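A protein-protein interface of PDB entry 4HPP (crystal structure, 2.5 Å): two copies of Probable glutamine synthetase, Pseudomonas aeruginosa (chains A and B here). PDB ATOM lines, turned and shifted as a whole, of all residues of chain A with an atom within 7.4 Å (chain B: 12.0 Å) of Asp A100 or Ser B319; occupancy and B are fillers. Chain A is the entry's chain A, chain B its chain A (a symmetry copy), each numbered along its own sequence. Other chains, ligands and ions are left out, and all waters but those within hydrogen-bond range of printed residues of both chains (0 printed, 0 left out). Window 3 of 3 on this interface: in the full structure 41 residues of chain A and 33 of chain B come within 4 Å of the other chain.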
ATOM      1  N   ALA A  36     -16.322  10.539  -5.516  1.00  0.00           N
ATOM      2  CA  ALA A  36     -15.586   9.258  -5.493  1.00  0.00           C
ATOM      3  C   ALA A  36     -15.264   8.708  -4.089  1.00  0.00           C
ATOM      4  O   ALA A  36     -15.253   7.472  -3.890  1.00  0.00           O
ATOM      5  CB  ALA A  36     -14.320   9.332  -6.350  1.00  0.00           C
ATOM      6  N   SER A  37     -15.003   9.614  -3.144  1.00  0.00           N
ATOM      7  CA  SER A  37     -14.632   9.255  -1.770  1.00  0.00           C
ATOM      8  C   SER A  37     -15.874   9.198  -0.883  1.00  0.00           C
ATOM      9  O   SER A  37     -15.838   8.629   0.189  1.00  0.00           O
ATOM     10  CB  SER A  37     -13.686  10.335  -1.175  1.00  0.00           C
ATOM     11  OG  SER A  37     -14.340  11.632  -1.115  1.00  0.00           O
ATOM     12  N   ARG A  67     -17.126   4.640   4.732  1.00  0.00           N
ATOM     13  CA  ARG A  67     -17.426   5.675   3.760  1.00  0.00           C
ATOM     14  C   ARG A  67     -18.882   5.588   3.372  1.00  0.00           C
ATOM     15  O   ARG A  67     -19.372   4.505   3.199  1.00  0.00           O
ATOM     16  CB  ARG A  67     -16.624   5.507   2.484  1.00  0.00           C
ATOM     17  CG  ARG A  67     -15.132   5.567   2.639  1.00  0.00           C
ATOM     18  CD  ARG A  67     -14.667   6.780   3.422  1.00  0.00           C
ATOM     19  NE  ARG A  67     -15.016   8.046   2.793  1.00  0.00           N
ATOM     20  CZ  ARG A  67     -14.617   9.221   3.265  1.00  0.00           C
ATOM     21  NH1 ARG A  67     -13.856   9.253   4.350  1.00  0.00           N
ATOM     22  NH2 ARG A  67     -14.985  10.352   2.674  1.00  0.00           N
ATOM     23  N   VAL A  97     -19.736   1.626   2.866  1.00  0.00           N
ATOM     24  CA  VAL A  97     -18.682   0.686   2.449  1.00  0.00           C
ATOM     25  C   VAL A  97     -17.491   0.878   3.365  1.00  0.00           C
ATOM     26  O   VAL A  97     -17.366   1.945   3.937  1.00  0.00           O
ATOM     27  CB  VAL A  97     -18.276   0.911   0.971  1.00  0.00           C
ATOM     28  CG1 VAL A  97     -19.497   0.791   0.092  1.00  0.00           C
ATOM     29  CG2 VAL A  97     -17.645   2.292   0.754  1.00  0.00           C
ATOM     30  N   GLU A  98     -16.642  -0.147   3.522  1.00  0.00           N
ATOM     31  CA  GLU A  98     -15.386  -0.042   4.319  1.00  0.00           C
ATOM     32  C   GLU A  98     -14.379   0.791   3.520  1.00  0.00           C
ATOM     33  O   GLU A  98     -14.666   1.077   2.359  1.00  0.00           O
ATOM     34  CB  GLU A  98     -14.875  -1.437   4.680  1.00  0.00           C
ATOM     35  CG  GLU A  98     -15.551  -2.039   5.934  1.00  0.00           C
ATOM     36  CD  GLU A  98     -16.274  -3.377   5.683  1.00  0.00           C
ATOM     37  OE1 GLU A  98     -15.948  -4.083   4.697  1.00  0.00           O
ATOM     38  OE2 GLU A  98     -17.186  -3.745   6.469  1.00  0.00           O
ATOM     39  N   THR A  99     -13.241   1.223   4.088  1.00  0.00           N
ATOM     40  CA  THR A  99     -12.415   2.296   3.396  1.00  0.00           C
ATOM     41  C   THR A  99     -11.803   1.966   2.011  1.00  0.00           C
ATOM     42  O   THR A  99     -11.476   2.880   1.236  1.00  0.00           O
ATOM     43  CB  THR A  99     -11.318   2.965   4.294  1.00  0.00           C
ATOM     44  OG1 THR A  99     -10.632   1.981   5.077  1.00  0.00           O
ATOM     45  CG2 THR A  99     -11.906   4.009   5.223  1.00  0.00           C
ATOM     46  N   ASP A 100     -11.666   0.667   1.728  1.00  0.00           N
ATOM     47  CA  ASP A 100     -11.093   0.116   0.471  1.00  0.00           C
ATOM     48  C   ASP A 100     -12.072   0.001  -0.710  1.00  0.00           C
ATOM     49  O   ASP A 100     -11.638  -0.246  -1.842  1.00  0.00           O
ATOM     50  CB  ASP A 100     -10.495  -1.293   0.730  1.00  0.00           C
ATOM     51  CG  ASP A 100     -11.410  -2.183   1.600  1.00  0.00           C
ATOM     52  OD1 ASP A 100     -10.906  -3.040   2.329  1.00  0.00           O
ATOM     53  OD2 ASP A 100     -12.641  -2.035   1.586  1.00  0.00           O
ATOM     54  N   GLY A 101     -13.377   0.148  -0.439  1.00  0.00           N
ATOM     55  CA  GLY A 101     -14.457  -0.074  -1.432  1.00  0.00           C
ATOM     56  C   GLY A 101     -15.455  -1.182  -1.072  1.00  0.00           C
ATOM     57  O   GLY A 101     -16.415  -1.442  -1.809  1.00  0.00           O
ATOM     58  N   THR A 102     -15.251  -1.803   0.088  1.00  0.00           N
ATOM     59  CA  THR A 102     -15.888  -3.078   0.421  1.00  0.00           C
ATOM     60  C   THR A 102     -17.294  -2.924   1.010  1.00  0.00           C
ATOM     61  O   THR A 102     -17.435  -2.424   2.146  1.00  0.00           O
ATOM     62  CB  THR A 102     -14.989  -3.904   1.375  1.00  0.00           C
ATOM     63  OG1 THR A 102     -13.696  -4.056   0.781  1.00  0.00           O
ATOM     64  CG2 THR A 102     -15.602  -5.294   1.700  1.00  0.00           C
ATOM     65  N   PRO A 103     -18.326  -3.374   0.243  1.00  0.00           N
ATOM     66  CA  PRO A 103     -19.728  -3.246   0.646  1.00  0.00           C
ATOM     67  C   PRO A 103     -19.936  -3.665   2.088  1.00  0.00           C
ATOM     68  O   PRO A 103     -19.662  -4.802   2.422  1.00  0.00           O
ATOM     69  CB  PRO A 103     -20.461  -4.190  -0.313  1.00  0.00           C
ATOM     70  CG  PRO A 103     -19.606  -4.200  -1.546  1.00  0.00           C
ATOM     71  CD  PRO A 103     -18.186  -3.977  -1.104  1.00  0.00           C
ATOM     72  N   TYR B 251       4.178   9.083   7.513  1.00  0.00           N
ATOM     73  CA  TYR B 251       3.592   7.860   6.958  1.00  0.00           C
ATOM     74  C   TYR B 251       4.486   6.977   6.073  1.00  0.00           C
ATOM     75  O   TYR B 251       5.184   7.461   5.179  1.00  0.00           O
ATOM     76  CB  TYR B 251       2.262   8.201   6.299  1.00  0.00           C
ATOM     77  CG  TYR B 251       1.849   7.394   5.088  1.00  0.00           C
ATOM     78  CD1 TYR B 251       2.354   7.697   3.815  1.00  0.00           C
ATOM     79  CD2 TYR B 251       0.894   6.374   5.201  1.00  0.00           C
ATOM     80  CE1 TYR B 251       1.952   6.974   2.698  1.00  0.00           C
ATOM     81  CE2 TYR B 251       0.481   5.649   4.096  1.00  0.00           C
ATOM     82  CZ  TYR B 251       1.016   5.960   2.848  1.00  0.00           C
ATOM     83  OH  TYR B 251       0.619   5.251   1.747  1.00  0.00           O
ATOM     84  N   PRO B 253       3.917   3.040   4.389  1.00  0.00           N
ATOM     85  CA  PRO B 253       3.165   1.786   4.210  1.00  0.00           C
ATOM     86  C   PRO B 253       3.959   0.616   4.774  1.00  0.00           C
ATOM     87  O   PRO B 253       5.189   0.701   4.858  1.00  0.00           O
ATOM     88  CB  PRO B 253       3.058   1.641   2.686  1.00  0.00           C
ATOM     89  CG  PRO B 253       3.249   3.015   2.141  1.00  0.00           C
ATOM     90  CD  PRO B 253       4.125   3.756   3.108  1.00  0.00           C
ATOM     91  N   ASP B 258       1.119   2.197   9.250  1.00  0.00           N
ATOM     92  CA  ASP B 258       1.652   3.044   8.156  1.00  0.00           C
ATOM     93  C   ASP B 258       2.380   4.242   8.768  1.00  0.00           C
ATOM     94  O   ASP B 258       2.591   5.261   8.105  1.00  0.00           O
ATOM     95  CB  ASP B 258       0.582   3.476   7.125  1.00  0.00           C
ATOM     96  CG  ASP B 258      -0.125   2.297   6.480  1.00  0.00           C
ATOM     97  OD1 ASP B 258       0.534   1.279   6.141  1.00  0.00           O
ATOM     98  OD2 ASP B 258      -1.351   2.399   6.293  1.00  0.00           O
ATOM     99  N   CYS B 315      -5.512   8.554  11.679  1.00  0.00           N
ATOM    100  CA  CYS B 315      -6.594   8.680  10.676  1.00  0.00           C
ATOM    101  C   CYS B 315      -6.106   8.072   9.379  1.00  0.00           C
ATOM    102  O   CYS B 315      -5.438   8.766   8.568  1.00  0.00           O
ATOM    103  CB  CYS B 315      -7.003  10.150  10.419  1.00  0.00           C
ATOM    104  SG  CYS B 315      -7.568  11.064  11.888  1.00  0.00           S
ATOM    105  N   PRO B 316      -6.453   6.789   9.165  1.00  0.00           N
ATOM    106  CA  PRO B 316      -5.848   6.051   8.077  1.00  0.00           C
ATOM    107  C   PRO B 316      -6.293   6.661   6.750  1.00  0.00           C
ATOM    108  O   PRO B 316      -7.240   7.461   6.708  1.00  0.00           O
ATOM    109  CB  PRO B 316      -6.417   4.643   8.253  1.00  0.00           C
ATOM    110  CG  PRO B 316      -7.778   4.870   8.841  1.00  0.00           C
ATOM    111  CD  PRO B 316      -7.742   6.200   9.569  1.00  0.00           C
ATOM    112  N   VAL B 317      -5.596   6.306   5.682  1.00  0.00           N
ATOM    113  CA  VAL B 317      -5.939   6.812   4.361  1.00  0.00           C
ATOM    114  C   VAL B 317      -7.278   6.234   3.803  1.00  0.00           C
ATOM    115  O   VAL B 317      -7.757   5.191   4.254  1.00  0.00           O
ATOM    116  CB  VAL B 317      -4.747   6.625   3.408  1.00  0.00           C
ATOM    117  CG1 VAL B 317      -3.643   7.618   3.781  1.00  0.00           C
ATOM    118  CG2 VAL B 317      -4.258   5.174   3.438  1.00  0.00           C
ATOM    119  N   VAL B 318      -7.905   6.949   2.866  1.00  0.00           N
ATOM    120  CA  VAL B 318      -9.066   6.425   2.112  1.00  0.00           C
ATOM    121  C   VAL B 318      -8.611   6.095   0.659  1.00  0.00           C
ATOM    122  O   VAL B 318      -8.285   7.009  -0.119  1.00  0.00           O
ATOM    123  CB  VAL B 318     -10.352   7.361   2.209  1.00  0.00           C
ATOM    124  CG1 VAL B 318     -10.273   8.307   3.400  1.00  0.00           C
ATOM    125  CG2 VAL B 318     -10.609   8.200   0.952  1.00  0.00           C
ATOM    126  N   SER B 319      -8.556   4.807   0.308  1.00  0.00           N
ATOM    127  CA  SER B 319      -8.242   4.431  -1.095  1.00  0.00           C
ATOM    128  C   SER B 319      -9.478   4.591  -1.974  1.00  0.00           C
ATOM    129  O   SER B 319      -9.625   5.598  -2.649  1.00  0.00           O
ATOM    130  CB  SER B 319      -7.608   3.033  -1.231  1.00  0.00           C
ATOM    131  OG  SER B 319      -8.266   2.080  -0.435  1.00  0.00           O
ATOM    132  N   VAL B 320     -10.370   3.610  -1.923  1.00  0.00           N
ATOM    133  CA  VAL B 320     -11.704   3.690  -2.502  1.00  0.00           C
ATOM    134  C   VAL B 320     -11.836   4.042  -4.019  1.00  0.00           C
ATOM    135  O   VAL B 320     -12.074   3.148  -4.846  1.00  0.00           O
ATOM    136  CB  VAL B 320     -12.643   4.505  -1.593  1.00  0.00           C
ATOM    137  CG1 VAL B 320     -12.588   6.007  -1.910  1.00  0.00           C
ATOM    138  CG2 VAL B 320     -14.046   3.927  -1.675  1.00  0.00           C
ATOM    139  N   GLY B 321     -11.692   5.316  -4.381  1.00  0.00           N
ATOM    140  CA  GLY B 321     -11.812   5.742  -5.780  1.00  0.00           C
ATOM    141  C   GLY B 321     -10.852   6.870  -6.107  1.00  0.00           C
ATOM    142  O   GLY B 321     -11.122   8.035  -5.801  1.00  0.00           O
ATOM    143  N   GLY B 322      -9.736   6.529  -6.749  1.00  0.00           N
ATOM    144  CA  GLY B 322      -8.613   7.453  -6.867  1.00  0.00           C
ATOM    145  C   GLY B 322      -8.021   7.556  -5.476  1.00  0.00           C
ATOM    146  O   GLY B 322      -7.904   6.544  -4.777  1.00  0.00           O
ATOM    147  N   LYS B 323      -7.667   8.775  -5.074  1.00  0.00           N
ATOM    148  CA  LYS B 323      -7.134   9.087  -3.732  1.00  0.00           C
ATOM    149  C   LYS B 323      -6.604  10.539  -3.732  1.00  0.00           C
ATOM    150  O   LYS B 323      -7.439  11.455  -3.783  1.00  0.00           O
ATOM    151  CB  LYS B 323      -6.086   8.074  -3.288  1.00  0.00           C
ATOM    152  N   PRO B 324      -5.250  10.770  -3.665  1.00  0.00           N
ATOM    153  CA  PRO B 324      -4.081   9.908  -3.296  1.00  0.00           C
ATOM    154  C   PRO B 324      -3.768   9.732  -1.777  1.00  0.00           C
ATOM    155  O   PRO B 324      -4.212  10.523  -0.931  1.00  0.00           O
ATOM    156  CB  PRO B 324      -2.896  10.547  -4.053  1.00  0.00           C
ATOM    157  CG  PRO B 324      -3.309  11.949  -4.330  1.00  0.00           C
ATOM    158  CD  PRO B 324      -4.811  11.954  -4.445  1.00  0.00           C
ATOM    159  N   LEU B 325      -2.991   8.694  -1.467  1.00  0.00           N
ATOM    160  CA  LEU B 325      -2.823   8.189  -0.092  1.00  0.00           C
ATOM    161  C   LEU B 325      -1.570   8.754   0.623  1.00  0.00           C
ATOM    162  O   LEU B 325      -0.486   8.828   0.038  1.00  0.00           O
ATOM    163  CB  LEU B 325      -2.802   6.631  -0.084  1.00  0.00           C
ATOM    164  CG  LEU B 325      -4.001   5.720  -0.452  1.00  0.00           C
ATOM    165  CD1 LEU B 325      -4.261   5.636  -1.953  1.00  0.00           C
ATOM    166  CD2 LEU B 325      -3.814   4.307   0.093  1.00  0.00           C
ATOM    167  N   GLY B 326      -1.706   9.149   1.888  1.00  0.00           N
ATOM    168  CA  GLY B 326      -0.538   9.587   2.631  1.00  0.00           C
ATOM    169  C   GLY B 326      -0.453  11.072   2.845  1.00  0.00           C
ATOM    170  O   GLY B 326      -0.158  11.521   3.947  1.00  0.00           O
ATOM    171  N   LYS B 327      -0.693  11.846   1.793  1.00  0.00           N
ATOM    172  CA  LYS B 327      -0.961  13.288   1.942  1.00  0.00           C
ATOM    173  C   LYS B 327      -2.125  13.505   2.929  1.00  0.00           C
ATOM    174  O   LYS B 327      -2.163  14.500   3.649  1.00  0.00           O
ATOM    175  CB  LYS B 327      -1.270  13.965   0.579  1.00  0.00           C
ATOM    176  CG  LYS B 327      -0.055  14.429  -0.250  1.00  0.00           C
ATOM    177  CD  LYS B 327       0.885  15.399   0.489  1.00  0.00           C
ATOM    178  CE  LYS B 327       1.229  16.665  -0.312  1.00  0.00           C
ATOM    179  NZ  LYS B 327       2.090  16.472  -1.522  1.00  0.00           N
ATOM    180  N   GLN B 328      -3.058  12.554   2.970  1.00  0.00           N
ATOM    181  CA  GLN B 328      -4.244  12.661   3.822  1.00  0.00           C
ATOM    182  C   GLN B 328      -4.045  11.917   5.148  1.00  0.00           C
ATOM    183  O   GLN B 328      -4.927  11.909   6.009  1.00  0.00           O
ATOM    184  CB  GLN B 328      -5.493  12.147   3.086  1.00  0.00           C
ATOM    185  CG  GLN B 328      -5.224  10.904   2.253  1.00  0.00           C
ATOM    186  CD  GLN B 328      -6.412   9.975   2.114  1.00  0.00           C
ATOM    187  OE1 GLN B 328      -7.031   9.600   3.112  1.00  0.00           O
ATOM    188  NE2 GLN B 328      -6.702   9.548   0.875  1.00  0.00           N
ATOM    189  N   TYR B 329      -2.880  11.295   5.305  1.00  0.00           N
ATOM    190  CA  TYR B 329      -2.532  10.594   6.532  1.00  0.00           C
ATOM    191  C   TYR B 329      -2.117  11.591   7.604  1.00  0.00           C
ATOM    192  O   TYR B 329      -1.262  12.482   7.389  1.00  0.00           O
ATOM    193  CB  TYR B 329      -1.391   9.636   6.273  1.00  0.00           C
ATOM    194  CG  TYR B 329      -1.054   8.768   7.449  1.00  0.00           C
ATOM    195  CD1 TYR B 329      -1.596   7.470   7.568  1.00  0.00           C
ATOM    196  CD2 TYR B 329      -0.165   9.226   8.435  1.00  0.00           C
ATOM    197  CE1 TYR B 329      -1.262   6.656   8.643  1.00  0.00           C
ATOM    198  CE2 TYR B 329       0.173   8.428   9.509  1.00  0.00           C
ATOM    199  CZ  TYR B 329      -0.374   7.150   9.611  1.00  0.00           C
ATOM    200  OH  TYR B 329      -0.012   6.404  10.694  1.00  0.00           O
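N of Val B320 lies within hydrogen-bond range of O of Thr A99.
The guanidinium group (NE) of Arg A67 lies within hydrogen-bond range of the backbone carbonyl oxygen (O) of Ser A37, 2.8 Å away.
The backbone NH of Arg A67 sits at hydrogen-bond distance from the backbone carbonyl oxygen of Val A97 (2.8 Å).
OD2 of Asp A100 sits at hydrogen-bond distance from OG1 of Thr A102, at 2.4 Å.
N of Val B318 lies within hydrogen-bond range of OE1 of Gln B328, 2.8 Å away.
Among the printed residues, merely in contact across the chains: Ala A36 with Val B320 (3.6 Å), Ala A36 with Gly B321 (3.5 Å), Ser A37 with Val B320 (3.8 Å), Arg A67 with Val B318 (3.8 Å), Thr A99 with Ser B319 (3.6 Å), Asp A100 with Ser B319 (3.6 Å) and Asp A100 with Val B320 (3.99 Å).
Printed residues of chain B within 4 Å of Ala A36: Val B320 (3.6 Å) and Gly B321 (3.5 Å).
Of chain B, only Val B320 comes within 4 Å of Ser A37.
Of the printed residues of chain B, Arg A67 touches Val B318 (3.8 Å).
No residue of chain B comes within 4 Å of Glu A98.
Of chain B, only Ser B319 (3.6 Å) and Val B320 (3.4 Å) come within 4 Å of Thr A99.
Printed residues of chain B within 4 Å of Asp A100: Ser B319 (3.6 Å) and Val B320 (3.99 Å).
Cys B315 touches none of the printed residues of chain A.
Of the printed residues of chain A, Val B318 touches Arg A67.
Ser B319 touches two residues of chain A.
Printed residues of chain A within 4 Å of Gly B321: Ala A36.
The nearest residue of chain A that does not touch Ser B319 is Gly A101 (5.5 Å).
The nearest printed residue of chain B that does not touch Ala A36 is Gly B322 (5.4 Å).
Of the 18 printed residues of chain B, 4 touch a printed residue of chain A.
Hydrophobic or aromatic side chains of chain B that line the printed part of chain A: Val B318 and Val B320.
Along chain A the printed residues that touch a printed residue of chain B span positions 36 to 100.
Among the printed residues, 8 pairs touch across the chains.
Among the printed residues, no Asp or Glu carboxylate lies within 4 Å of a Lys or Arg side-chain nitrogen of the other chain.
No position is printed for both chains.
Of the 8 pairs that touch across the chains among the printed residues, none has its exchanged pair printed and touching as well.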
